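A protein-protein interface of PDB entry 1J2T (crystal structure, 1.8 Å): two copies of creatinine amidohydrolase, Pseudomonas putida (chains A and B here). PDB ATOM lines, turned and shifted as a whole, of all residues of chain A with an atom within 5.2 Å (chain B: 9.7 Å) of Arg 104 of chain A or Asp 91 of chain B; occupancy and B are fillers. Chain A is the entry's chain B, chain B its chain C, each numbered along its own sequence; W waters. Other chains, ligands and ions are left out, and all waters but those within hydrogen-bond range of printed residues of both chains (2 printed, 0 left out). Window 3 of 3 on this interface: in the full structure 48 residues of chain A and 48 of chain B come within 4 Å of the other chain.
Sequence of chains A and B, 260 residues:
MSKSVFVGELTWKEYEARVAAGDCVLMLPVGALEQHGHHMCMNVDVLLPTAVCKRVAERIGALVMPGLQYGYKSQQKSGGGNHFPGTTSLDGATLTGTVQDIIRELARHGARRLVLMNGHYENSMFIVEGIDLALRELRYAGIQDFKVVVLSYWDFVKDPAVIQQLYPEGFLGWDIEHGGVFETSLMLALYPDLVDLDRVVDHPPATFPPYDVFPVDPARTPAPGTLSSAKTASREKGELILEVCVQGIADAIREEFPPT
Of the 12 printed residues of chain A, 5 touch a printed residue of chain B.
Printed residues of chain A that touch a printed residue of chain B: Asp 101, Ile 102, Arg 104, Glu 105 and Arg 108.
Hydrophobic or aromatic side chains of chain A within 4 Å of the printed part of chain B: Ile 102.
Printed residues of chain B that touch a printed residue of chain A: Tyr 70, Asn 82, Phe 84, Thr 87, Thr 88, Ser 89, Leu 90, Asp 91 and Thr 94.
Among the printed residues, 13 pairs touch across the chains.
Among the printed residues, pairs that only touch across the chains: Asp 101 of chain A with Leu 90 of chain B, Glu 105 of chain A with Thr 87 of chain B, Glu 105 of chain A with Thr 88 of chain B, Ile 102 of chain A with Tyr 70 of chain B and Asp 101 of chain A with Ser 89 of chain B.
The side-chain carboxylate (OD2) of Asp 101 of chain A is in hydrogen-bond range of the backbone NH (N) of Asp 91 of chain B (2.9 Å).
OG1 of Thr 94 of chain B lies within hydrogen-bond range of OD2 of Asp 101 of chain A (2.6 Å).
NH2 of Arg 104 of chain A is in salt-bridge range of OD2 of Asp 91 of chain B (3.4 Å).
The side-chain amide oxygen of Asn 82 of chain B sits close to the side-chain carboxylate of Glu 105 of chain A (3.0 Å).
OE1 of Glu 105 of chain A is in hydrogen-bond range of N of Ser 89 of chain B (2.8 Å).
The guanidinium group (NH1) of Arg 108 of chain A sits close to the backbone carbonyl oxygen (O) of Asn 82 of chain B, at 3.1 Å.
The backbone carbonyl oxygen (O) of Phe 84 of chain B sits at hydrogen-bond distance from the guanidinium group (NH1) of Arg 108 of chain A (3.0 Å).
NH2 of Arg 108 of chain A lies within hydrogen-bond range of O of Thr 87 of chain B.
Position printed for both chains: 99.
Of the 13 pairs that touch across the chains among the printed residues, none has its exchanged pair printed and touching as well.
Water W2 lies within hydrogen-bond range of the side-chain carboxylate of Asp 91 of chain B, the guanidinium group of Arg 104 of chain A and the side-chain carboxylate of Asp 101 of chain A.
Water W1 lies within hydrogen-bond range of O of Ser 89 of chain B (2.8 Å), OD2 of Asp 91 of chain B (3.0 Å) and NH2 of Arg 104 of chain A (3.1 Å).
The side-chain carboxylate (OD1) of Asp 101 of chain A is in salt-bridge range of the guanidinium group (NH2) of Arg 104 of chain A, 2.9 Å away.
The side-chain carboxylate (OE1) of Glu 137 of chain A lies within salt-bridge range of the guanidinium group (NH1) of Arg 104 of chain A, at 3.1 Å.
N of Leu 90 of chain B sits at hydrogen-bond distance from O of Gly 71 of chain B (2.8 Å).
NZ of Lys 73 of chain B is in salt-bridge range of OD2 of Asp 91 of chain B.
The backbone NH (N) of Ser 74 of chain B lies close to the side-chain amide nitrogen (ND2) of Asn 82 of chain B.
OG1 of Thr 98 of chain B sits at hydrogen-bond distance from O of Thr 94 of chain B (2.8 Å).
Printed residues of chain B within 4 Å of Ile 102 of chain A: Tyr 70.
Of the printed residues of chain B, Glu 105 of chain A touches Asn 82 (3.0 Å), Thr 87 (3.5 Å), Thr 88 (3.6 Å) and Ser 89 (2.8 Å).
No residue of chain B comes within 4 Å of Ala 107 of chain A.
Gly 71 of chain B touches none of the printed residues of chain A.
Printed residues of chain A within 4 Å of Asn 82 of chain B: Glu 105 (3.0 Å) and Arg 108 (2.9 Å).
Of the printed residues of chain A, Leu 90 of chain B touches Asp 101 (3.5 Å).
Of chain A, only Asp 101 and Arg 104 come within 4 Å of Asp 91 of chain B.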
ATOM      1  N   VAL A  99       8.001  30.147   1.879  1.00  0.00           N
ATOM      2  CA  VAL A  99       7.878  29.710   0.496  1.00  0.00           C
ATOM      3  C   VAL A  99       7.983  28.177   0.417  1.00  0.00           C
ATOM      4  O   VAL A  99       7.185  27.522  -0.263  1.00  0.00           O
ATOM      5  CB  VAL A  99       8.942  30.388  -0.401  1.00  0.00           C
ATOM      6  CG1 VAL A  99       8.987  29.746  -1.773  1.00  0.00           C
ATOM      7  CG2 VAL A  99       8.665  31.876  -0.528  1.00  0.00           C
ATOM      8  N   GLN A 100       8.938  27.612   1.144  1.00  0.00           N
ATOM      9  CA  GLN A 100       9.160  26.182   1.171  1.00  0.00           C
ATOM     10  C   GLN A 100       7.918  25.435   1.695  1.00  0.00           C
ATOM     11  O   GLN A 100       7.470  24.456   1.089  1.00  0.00           O
ATOM     12  CB  GLN A 100      10.399  25.876   2.037  1.00  0.00           C
ATOM     13  CG  GLN A 100      10.702  24.422   2.267  1.00  0.00           C
ATOM     14  CD  GLN A 100      11.913  24.235   3.175  1.00  0.00           C
ATOM     15  OE1 GLN A 100      12.416  25.214   3.733  1.00  0.00           O
ATOM     16  NE2 GLN A 100      12.356  22.981   3.364  1.00  0.00           N
ATOM     17  N   ASP A 101       7.352  25.905   2.807  1.00  0.00           N
ATOM     18  CA  ASP A 101       6.192  25.255   3.393  1.00  0.00           C
ATOM     19  C   ASP A 101       4.997  25.302   2.443  1.00  0.00           C
ATOM     20  O   ASP A 101       4.269  24.318   2.293  1.00  0.00           O
ATOM     21  CB  ASP A 101       5.766  25.936   4.695  1.00  0.00           C
ATOM     22  CG  ASP A 101       6.754  25.754   5.836  1.00  0.00           C
ATOM     23  OD1 ASP A 101       7.728  24.965   5.729  1.00  0.00           O
ATOM     24  OD2 ASP A 101       6.613  26.402   6.907  1.00  0.00           O
ATOM     25  N   ILE A 102       4.798  26.439   1.791  1.00  0.00           N
ATOM     26  CA  ILE A 102       3.649  26.584   0.899  1.00  0.00           C
ATOM     27  C   ILE A 102       3.751  25.631  -0.268  1.00  0.00           C
ATOM     28  O   ILE A 102       2.770  24.978  -0.594  1.00  0.00           O
ATOM     29  CB  ILE A 102       3.474  28.043   0.443  1.00  0.00           C
ATOM     30  CG1 ILE A 102       2.965  28.877   1.628  1.00  0.00           C
ATOM     31  CG2 ILE A 102       2.475  28.127  -0.688  1.00  0.00           C
ATOM     32  CD1 ILE A 102       3.111  30.366   1.447  1.00  0.00           C
ATOM     33  N   ILE A 103       4.932  25.518  -0.876  1.00  0.00           N
ATOM     34  CA  ILE A 103       5.104  24.601  -2.009  1.00  0.00           C
ATOM     35  C   ILE A 103       4.856  23.162  -1.593  1.00  0.00           C
ATOM     36  O   ILE A 103       4.187  22.401  -2.317  1.00  0.00           O
ATOM     37  CB  ILE A 103       6.492  24.759  -2.646  1.00  0.00           C
ATOM     38  CG1 ILE A 103       6.580  26.133  -3.296  1.00  0.00           C
ATOM     39  CG2 ILE A 103       6.745  23.651  -3.691  1.00  0.00           C
ATOM     40  CD1 ILE A 103       7.965  26.541  -3.714  1.00  0.00           C
ATOM     41  N   ARG A 104       5.409  22.775  -0.444  1.00  0.00           N
ATOM     42  CA  ARG A 104       5.182  21.434   0.107  1.00  0.00           C
ATOM     43  C   ARG A 104       3.685  21.136   0.145  1.00  0.00           C
ATOM     44  O   ARG A 104       3.212  20.080  -0.301  1.00  0.00           O
ATOM     45  CB  ARG A 104       5.741  21.345   1.533  1.00  0.00           C
ATOM     46  CG  ARG A 104       5.515  19.997   2.231  1.00  0.00           C
ATOM     47  CD  ARG A 104       5.980  19.956   3.697  1.00  0.00           C
ATOM     48  NE  ARG A 104       7.371  20.338   3.816  1.00  0.00           N
ATOM     49  CZ  ARG A 104       7.827  21.399   4.477  1.00  0.00           C
ATOM     50  NH1 ARG A 104       9.121  21.643   4.471  1.00  0.00           N
ATOM     51  NH2 ARG A 104       7.015  22.193   5.168  1.00  0.00           N
ATOM     52  N   GLU A 105       2.937  22.084   0.691  1.00  0.00           N
ATOM     53  CA  GLU A 105       1.492  21.929   0.859  1.00  0.00           C
ATOM     54  C   GLU A 105       0.741  21.880  -0.466  1.00  0.00           C
ATOM     55  O   GLU A 105      -0.149  21.031  -0.650  1.00  0.00           O
ATOM     56  CB  GLU A 105       0.970  23.046   1.760  1.00  0.00           C
ATOM     57  CG  GLU A 105       1.384  22.857   3.208  1.00  0.00           C
ATOM     58  CD  GLU A 105       0.529  21.816   3.920  1.00  0.00           C
ATOM     59  OE1 GLU A 105      -0.515  22.193   4.485  1.00  0.00           O
ATOM     60  OE2 GLU A 105       0.884  20.627   3.899  1.00  0.00           O
ATOM     61  N   LEU A 106       1.089  22.779  -1.389  1.00  0.00           N
ATOM     62  CA  LEU A 106       0.495  22.743  -2.726  1.00  0.00           C
ATOM     63  C   LEU A 106       0.737  21.399  -3.403  1.00  0.00           C
ATOM     64  O   LEU A 106      -0.169  20.828  -4.020  1.00  0.00           O
ATOM     65  CB  LEU A 106       1.029  23.889  -3.595  1.00  0.00           C
ATOM     66  CG  LEU A 106       0.587  25.284  -3.134  1.00  0.00           C
ATOM     67  CD1 LEU A 106       1.124  26.364  -4.068  1.00  0.00           C
ATOM     68  CD2 LEU A 106      -0.929  25.392  -2.993  1.00  0.00           C
ATOM     69  N   ALA A 107       1.944  20.871  -3.269  1.00  0.00           N
ATOM     70  CA  ALA A 107       2.268  19.575  -3.850  1.00  0.00           C
ATOM     71  C   ALA A 107       1.411  18.459  -3.219  1.00  0.00           C
ATOM     72  O   ALA A 107       0.921  17.552  -3.917  1.00  0.00           O
ATOM     73  CB  ALA A 107       3.760  19.281  -3.693  1.00  0.00           C
ATOM     74  N   ARG A 108       1.194  18.553  -1.908  1.00  0.00           N
ATOM     75  CA  ARG A 108       0.346  17.596  -1.204  1.00  0.00           C
ATOM     76  C   ARG A 108      -1.067  17.578  -1.790  1.00  0.00           C
ATOM     77  O   ARG A 108      -1.687  16.508  -1.901  1.00  0.00           O
ATOM     78  CB  ARG A 108       0.281  17.929   0.283  1.00  0.00           C
ATOM     79  CG  ARG A 108      -0.647  17.031   1.084  1.00  0.00           C
ATOM     80  CD  ARG A 108      -0.636  17.319   2.567  1.00  0.00           C
ATOM     81  NE  ARG A 108      -1.075  18.672   2.922  1.00  0.00           N
ATOM     82  CZ  ARG A 108      -2.324  19.124   2.825  1.00  0.00           C
ATOM     83  NH1 ARG A 108      -3.293  18.358   2.344  1.00  0.00           N
ATOM     84  NH2 ARG A 108      -2.604  20.361   3.209  1.00  0.00           N
ATOM     85  N   ALA A 134      12.110  23.162  -1.318  1.00  0.00           N
ATOM     86  CA  ALA A 134      10.863  22.412  -1.503  1.00  0.00           C
ATOM     87  C   ALA A 134      11.004  21.367  -2.628  1.00  0.00           C
ATOM     88  O   ALA A 134      10.527  20.226  -2.506  1.00  0.00           O
ATOM     89  CB  ALA A 134       9.711  23.338  -1.778  1.00  0.00           C
ATOM     90  N   GLU A 137      12.872  18.265  -1.370  1.00  0.00           N
ATOM     91  CA  GLU A 137      12.020  17.360  -0.612  1.00  0.00           C
ATOM     92  C   GLU A 137      11.116  16.541  -1.551  1.00  0.00           C
ATOM     93  O   GLU A 137      10.873  15.348  -1.334  1.00  0.00           O
ATOM     94  CB  GLU A 137      11.166  18.146   0.385  1.00  0.00           C
ATOM     95  CG  GLU A 137      11.993  18.786   1.487  1.00  0.00           C
ATOM     96  CD  GLU A 137      11.186  19.719   2.368  1.00  0.00           C
ATOM     97  OE1 GLU A 137      10.029  20.007   2.043  1.00  0.00           O
ATOM     98  OE2 GLU A 137      11.731  20.146   3.383  1.00  0.00           O
ATOM     99  N   TYR B  70      -1.107  32.508   6.591  1.00  0.00           N
ATOM    100  CA  TYR B  70      -0.876  31.081   6.738  1.00  0.00           C
ATOM    101  C   TYR B  70      -0.513  30.787   8.180  1.00  0.00           C
ATOM    102  O   TYR B  70       0.326  31.477   8.770  1.00  0.00           O
ATOM    103  CB  TYR B  70       0.257  30.641   5.814  1.00  0.00           C
ATOM    104  CG  TYR B  70      -0.009  30.934   4.353  1.00  0.00           C
ATOM    105  CD1 TYR B  70       0.384  32.135   3.774  1.00  0.00           C
ATOM    106  CD2 TYR B  70      -0.651  29.999   3.540  1.00  0.00           C
ATOM    107  CE1 TYR B  70       0.131  32.402   2.411  1.00  0.00           C
ATOM    108  CE2 TYR B  70      -0.904  30.257   2.196  1.00  0.00           C
ATOM    109  CZ  TYR B  70      -0.514  31.464   1.636  1.00  0.00           C
ATOM    110  OH  TYR B  70      -0.759  31.701   0.284  1.00  0.00           O
ATOM    111  N   GLY B  71      -1.156  29.771   8.732  1.00  0.00           N
ATOM    112  CA  GLY B  71      -0.970  29.364  10.109  1.00  0.00           C
ATOM    113  C   GLY B  71      -0.501  27.934  10.255  1.00  0.00           C
ATOM    114  O   GLY B  71      -0.170  27.239   9.272  1.00  0.00           O
ATOM    115  N   TYR B  72      -0.488  27.480  11.503  1.00  0.00           N
ATOM    116  CA  TYR B  72      -0.058  26.134  11.811  1.00  0.00           C
ATOM    117  C   TYR B  72      -1.016  25.054  11.285  1.00  0.00           C
ATOM    118  O   TYR B  72      -2.202  25.289  11.034  1.00  0.00           O
ATOM    119  CB  TYR B  72       0.193  25.972  13.321  1.00  0.00           C
ATOM    120  CG  TYR B  72       0.824  24.635  13.621  1.00  0.00           C
ATOM    121  CD1 TYR B  72       2.089  24.325  13.133  1.00  0.00           C
ATOM    122  CD2 TYR B  72       0.127  23.652  14.299  1.00  0.00           C
ATOM    123  CE1 TYR B  72       2.663  23.084  13.361  1.00  0.00           C
ATOM    124  CE2 TYR B  72       0.681  22.406  14.524  1.00  0.00           C
ATOM    125  CZ  TYR B  72       1.951  22.122  14.045  1.00  0.00           C
ATOM    126  OH  TYR B  72       2.507  20.876  14.250  1.00  0.00           O
ATOM    127  N   LYS B  73      -0.452  23.869  11.095  1.00  0.00           N
ATOM    128  CA  LYS B  73      -1.146  22.690  10.596  1.00  0.00           C
ATOM    129  C   LYS B  73      -2.454  22.442  11.325  1.00  0.00           C
ATOM    130  O   LYS B  73      -2.485  22.393  12.549  1.00  0.00           O
ATOM    131  CB  LYS B  73      -0.243  21.467  10.749  1.00  0.00           C
ATOM    132  CG  LYS B  73       0.988  21.514   9.884  1.00  0.00           C
ATOM    133  CD  LYS B  73       2.158  20.742  10.460  1.00  0.00           C
ATOM    134  CE  LYS B  73       3.454  21.165   9.767  1.00  0.00           C
ATOM    135  NZ  LYS B  73       4.661  20.444  10.267  1.00  0.00           N
ATOM    136  N   SER B  74      -3.516  22.278  10.545  1.00  0.00           N
ATOM    137  CA  SER B  74      -4.852  21.996  11.048  1.00  0.00           C
ATOM    138  C   SER B  74      -4.846  20.669  11.811  1.00  0.00           C
ATOM    139  O   SER B  74      -4.256  19.684  11.351  1.00  0.00           O
ATOM    140  CB  SER B  74      -5.817  21.928   9.868  1.00  0.00           C
ATOM    141  OG  SER B  74      -7.134  21.558  10.261  1.00  0.00           O
ATOM    142  N   ASN B  82      -5.027  18.273   8.654  1.00  0.00           N
ATOM    143  CA  ASN B  82      -4.208  18.820   7.584  1.00  0.00           C
ATOM    144  C   ASN B  82      -4.170  17.962   6.323  1.00  0.00           C
ATOM    145  O   ASN B  82      -3.422  18.271   5.405  1.00  0.00           O
ATOM    146  CB  ASN B  82      -2.777  19.059   8.073  1.00  0.00           C
ATOM    147  CG  ASN B  82      -2.140  20.259   7.409  1.00  0.00           C
ATOM    148  OD1 ASN B  82      -1.174  20.138   6.626  1.00  0.00           O
ATOM    149  ND2 ASN B  82      -2.664  21.420   7.716  1.00  0.00           N
ATOM    150  N   PHE B  84      -6.804  17.605   4.394  1.00  0.00           N
ATOM    151  CA  PHE B  84      -7.717  18.210   3.426  1.00  0.00           C
ATOM    152  C   PHE B  84      -6.996  19.008   2.362  1.00  0.00           C
ATOM    153  O   PHE B  84      -5.958  19.603   2.617  1.00  0.00           O
ATOM    154  CB  PHE B  84      -8.708  19.156   4.100  1.00  0.00           C
ATOM    155  CG  PHE B  84      -9.888  18.453   4.691  1.00  0.00           C
ATOM    156  CD1 PHE B  84      -9.800  17.872   5.938  1.00  0.00           C
ATOM    157  CD2 PHE B  84     -11.074  18.345   3.982  1.00  0.00           C
ATOM    158  CE1 PHE B  84     -10.886  17.204   6.484  1.00  0.00           C
ATOM    159  CE2 PHE B  84     -12.159  17.676   4.522  1.00  0.00           C
ATOM    160  CZ  PHE B  84     -12.066  17.105   5.769  1.00  0.00           C
ATOM    161  N   THR B  87      -6.325  23.554   2.515  1.00  0.00           N
ATOM    162  CA  THR B  87      -5.594  23.912   3.727  1.00  0.00           C
ATOM    163  C   THR B  87      -4.113  23.950   3.398  1.00  0.00           C
ATOM    164  O   THR B  87      -3.563  22.967   2.891  1.00  0.00           O
ATOM    165  CB  THR B  87      -5.862  22.863   4.807  1.00  0.00           C
ATOM    166  OG1 THR B  87      -7.264  22.848   5.102  1.00  0.00           O
ATOM    167  CG2 THR B  87      -5.187  23.230   6.116  1.00  0.00           C
ATOM    168  N   THR B  88      -3.470  25.075   3.690  1.00  0.00           N
ATOM    169  CA  THR B  88      -2.061  25.290   3.358  1.00  0.00           C
ATOM    170  C   THR B  88      -1.367  25.790   4.609  1.00  0.00           C
ATOM    171  O   THR B  88      -1.515  26.961   4.979  1.00  0.00           O
ATOM    172  CB  THR B  88      -1.962  26.340   2.230  1.00  0.00           C
ATOM    173  OG1 THR B  88      -2.715  25.901   1.092  1.00  0.00           O
ATOM    174  CG2 THR B  88      -0.538  26.451   1.728  1.00  0.00           C
ATOM    175  N   SER B  89      -0.599  24.910   5.252  1.00  0.00           N
ATOM    176  CA  SER B  89      -0.061  25.206   6.577  1.00  0.00           C
ATOM    177  C   SER B  89       1.444  25.328   6.679  1.00  0.00           C
ATOM    178  O   SER B  89       2.197  24.660   5.951  1.00  0.00           O
ATOM    179  CB  SER B  89      -0.513  24.102   7.535  1.00  0.00           C
ATOM    180  OG  SER B  89      -1.918  23.906   7.443  1.00  0.00           O
ATOM    181  N   LEU B  90       1.868  26.152   7.630  1.00  0.00           N
ATOM    182  CA  LEU B  90       3.270  26.352   7.935  1.00  0.00           C
ATOM    183  C   LEU B  90       3.758  25.366   8.992  1.00  0.00           C
ATOM    184  O   LEU B  90       2.976  24.846   9.803  1.00  0.00           O
ATOM    185  CB  LEU B  90       3.510  27.767   8.463  1.00  0.00           C
ATOM    186  CG  LEU B  90       3.029  28.906   7.565  1.00  0.00           C
ATOM    187  CD1 LEU B  90       3.455  30.211   8.157  1.00  0.00           C
ATOM    188  CD2 LEU B  90       3.557  28.714   6.152  1.00  0.00           C
ATOM    189  N   ASP B  91       5.057  25.111   8.967  1.00  0.00           N
ATOM    190  CA  ASP B  91       5.704  24.394  10.038  1.00  0.00           C
ATOM    191  C   ASP B  91       5.723  25.317  11.259  1.00  0.00           C
ATOM    192  O   ASP B  91       5.665  26.540  11.137  1.00  0.00           O
ATOM    193  CB  ASP B  91       7.132  23.992   9.675  1.00  0.00           C
ATOM    194  CG  ASP B  91       7.190  22.744   8.852  1.00  0.00           C
ATOM    195  OD1 ASP B  91       8.317  22.309   8.505  1.00  0.00           O
ATOM    196  OD2 ASP B  91       6.154  22.135   8.495  1.00  0.00           O
ATOM    197  N   GLY B  92       5.785  24.720  12.438  1.00  0.00           N
ATOM    198  CA  GLY B  92       5.836  25.491  13.668  1.00  0.00           C
ATOM    199  C   GLY B  92       6.960  26.514  13.695  1.00  0.00           C
ATOM    200  O   GLY B  92       6.744  27.664  14.065  1.00  0.00           O
ATOM    201  N   ALA B  93       8.161  26.115  13.289  1.00  0.00           N
ATOM    202  CA  ALA B  93       9.303  27.019  13.325  1.00  0.00           C
ATOM    203  C   ALA B  93       9.100  28.238  12.429  1.00  0.00           C
ATOM    204  O   ALA B  93       9.596  29.307  12.728  1.00  0.00           O
ATOM    205  CB  ALA B  93      10.563  26.296  12.933  1.00  0.00           C
ATOM    206  N   THR B  94       8.408  28.038  11.316  1.00  0.00           N
ATOM    207  CA  THR B  94       8.159  29.102  10.360  1.00  0.00           C
ATOM    208  C   THR B  94       7.222  30.141  10.956  1.00  0.00           C
ATOM    209  O   THR B  94       7.459  31.346  10.857  1.00  0.00           O
ATOM    210  CB  THR B  94       7.523  28.525   9.092  1.00  0.00           C
ATOM    211  OG1 THR B  94       8.299  27.423   8.599  1.00  0.00           O
ATOM    212  CG2 THR B  94       7.547  29.540   7.967  1.00  0.00           C
ATOM    213  N   LEU B  95       6.152  29.673  11.570  1.00  0.00           N
ATOM    214  CA  LEU B  95       5.189  30.587  12.150  1.00  0.00           C
ATOM    215  C   LEU B  95       5.822  31.322  13.325  1.00  0.00           C
ATOM    216  O   LEU B  95       5.705  32.537  13.449  1.00  0.00           O
ATOM    217  CB  LEU B  95       3.944  29.825  12.577  1.00  0.00           C
ATOM    218  CG  LEU B  95       2.857  30.648  13.260  1.00  0.00           C
ATOM    219  CD1 LEU B  95       2.432  31.854  12.436  1.00  0.00           C
ATOM    220  CD2 LEU B  95       1.654  29.746  13.554  1.00  0.00           C
ATOM    221  N   THR B  96       6.491  30.577  14.192  1.00  0.00           N
ATOM    222  CA  THR B  96       7.175  31.152  15.341  1.00  0.00           C
ATOM    223  C   THR B  96       8.152  32.252  14.893  1.00  0.00           C
ATOM    224  O   THR B  96       8.189  33.351  15.438  1.00  0.00           O
ATOM    225  CB  THR B  96       7.914  30.034  16.078  1.00  0.00           C
ATOM    226  OG1 THR B  96       6.969  29.192  16.782  1.00  0.00           O
ATOM    227  CG2 THR B  96       8.829  30.584  17.148  1.00  0.00           C
ATOM    228  N   GLY B  97       8.950  31.952  13.882  1.00  0.00           N
ATOM    229  CA  GLY B  97       9.921  32.915  13.386  1.00  0.00           C
ATOM    230  C   GLY B  97       9.301  34.171  12.782  1.00  0.00           C
ATOM    231  O   GLY B  97       9.878  35.268  12.873  1.00  0.00           O
ATOM    232  N   THR B  98       8.141  34.020  12.161  1.00  0.00           N
ATOM    233  CA  THR B  98       7.443  35.151  11.559  1.00  0.00           C
ATOM    234  C   THR B  98       7.005  36.135  12.650  1.00  0.00           C
ATOM    235  O   THR B  98       7.216  37.348  12.550  1.00  0.00           O
ATOM    236  CB  THR B  98       6.255  34.654  10.747  1.00  0.00           C
ATOM    237  OG1 THR B  98       6.723  33.808   9.676  1.00  0.00           O
ATOM    238  CG2 THR B  98       5.545  35.787  10.047  1.00  0.00           C
ATOM    239  N   VAL B  99       6.401  35.592  13.697  1.00  0.00           N
ATOM    240  CA  VAL B  99       5.972  36.394  14.819  1.00  0.00           C
ATOM    241  C   VAL B  99       7.181  37.072  15.468  1.00  0.00           C
ATOM    242  O   VAL B  99       7.142  38.264  15.771  1.00  0.00           O
ATOM    243  CB  VAL B  99       5.195  35.511  15.834  1.00  0.00           C
ATOM    244  CG1 VAL B  99       5.022  36.213  17.144  1.00  0.00           C
ATOM    245  CG2 VAL B  99       3.845  35.116  15.258  1.00  0.00           C
ATOM    246  N   GLU B 122      -5.137  26.435  16.282  1.00  0.00           N
ATOM    247  CA  GLU B 122      -3.853  25.726  16.216  1.00  0.00           C
ATOM    248  C   GLU B 122      -2.617  26.631  16.305  1.00  0.00           C
ATOM    249  O   GLU B 122      -1.532  26.169  16.635  1.00  0.00           O
ATOM    250  CB  GLU B 122      -3.795  24.900  14.926  1.00  0.00           C
ATOM    251  CG  GLU B 122      -4.704  23.677  14.889  1.00  0.00           C
ATOM    252  CD  GLU B 122      -6.119  23.953  14.407  1.00  0.00           C
ATOM    253  OE1 GLU B 122      -6.574  25.107  14.499  1.00  0.00           O
ATOM    254  OE2 GLU B 122      -6.797  22.998  13.967  1.00  0.00           O
ATOM    255  N   ASN B 123      -2.775  27.919  16.022  1.00  0.00           N
ATOM    256  CA  ASN B 123      -1.647  28.835  16.046  1.00  0.00           C
ATOM    257  C   ASN B 123      -1.104  29.166  17.424  1.00  0.00           C
ATOM    258  O   ASN B 123       0.041  29.592  17.546  1.00  0.00           O
ATOM    259  CB  ASN B 123      -2.054  30.186  15.460  1.00  0.00           C
ATOM    260  CG  ASN B 123      -2.245  30.163  13.962  1.00  0.00           C
ATOM    261  OD1 ASN B 123      -1.732  29.293  13.260  1.00  0.00           O
ATOM    262  ND2 ASN B 123      -3.008  31.141  13.461  1.00  0.00           N
ATOM    263  N   PHE B 126       2.541  28.415  18.968  1.00  0.00           N
ATOM    264  CA  PHE B 126       3.616  28.925  18.122  1.00  0.00           C
ATOM    265  C   PHE B 126       3.686  30.448  18.215  1.00  0.00           C
ATOM    266  O   PHE B 126       4.773  31.028  18.155  1.00  0.00           O
ATOM    267  CB  PHE B 126       3.449  28.367  16.711  1.00  0.00           C
ATOM    268  CG  PHE B 126       3.409  26.880  16.710  1.00  0.00           C
ATOM    269  CD1 PHE B 126       2.201  26.205  16.670  1.00  0.00           C
ATOM    270  CD2 PHE B 126       4.572  26.158  16.899  1.00  0.00           C
ATOM    271  CE1 PHE B 126       2.161  24.820  16.751  1.00  0.00           C
ATOM    272  CE2 PHE B 126       4.537  24.773  16.971  1.00  0.00           C
ATOM    273  CZ  PHE B 126       3.322  24.110  16.895  1.00  0.00           C
ATOM    274  N   ILE B 127       2.537  31.080  18.441  1.00  0.00           N
ATOM    275  CA  ILE B 127       2.486  32.508  18.705  1.00  0.00           C
ATOM    276  C   ILE B 127       3.205  32.782  20.020  1.00  0.00           C
ATOM    277  O   ILE B 127       4.043  33.672  20.128  1.00  0.00           O
ATOM    278  CB  ILE B 127       1.036  32.982  18.795  1.00  0.00           C
ATOM    279  CG1 ILE B 127       0.400  33.019  17.405  1.00  0.00           C
ATOM    280  CG2 ILE B 127       0.985  34.350  19.458  1.00  0.00           C
ATOM    281  CD1 ILE B 127      -1.117  33.266  17.432  1.00  0.00           C
HETATM  282  O   HOH W   1       4.188  22.784   6.334  1.00  0.00           O
HETATM  283  O   HOH W   2      10.331  23.022   6.756  1.00  0.00           O
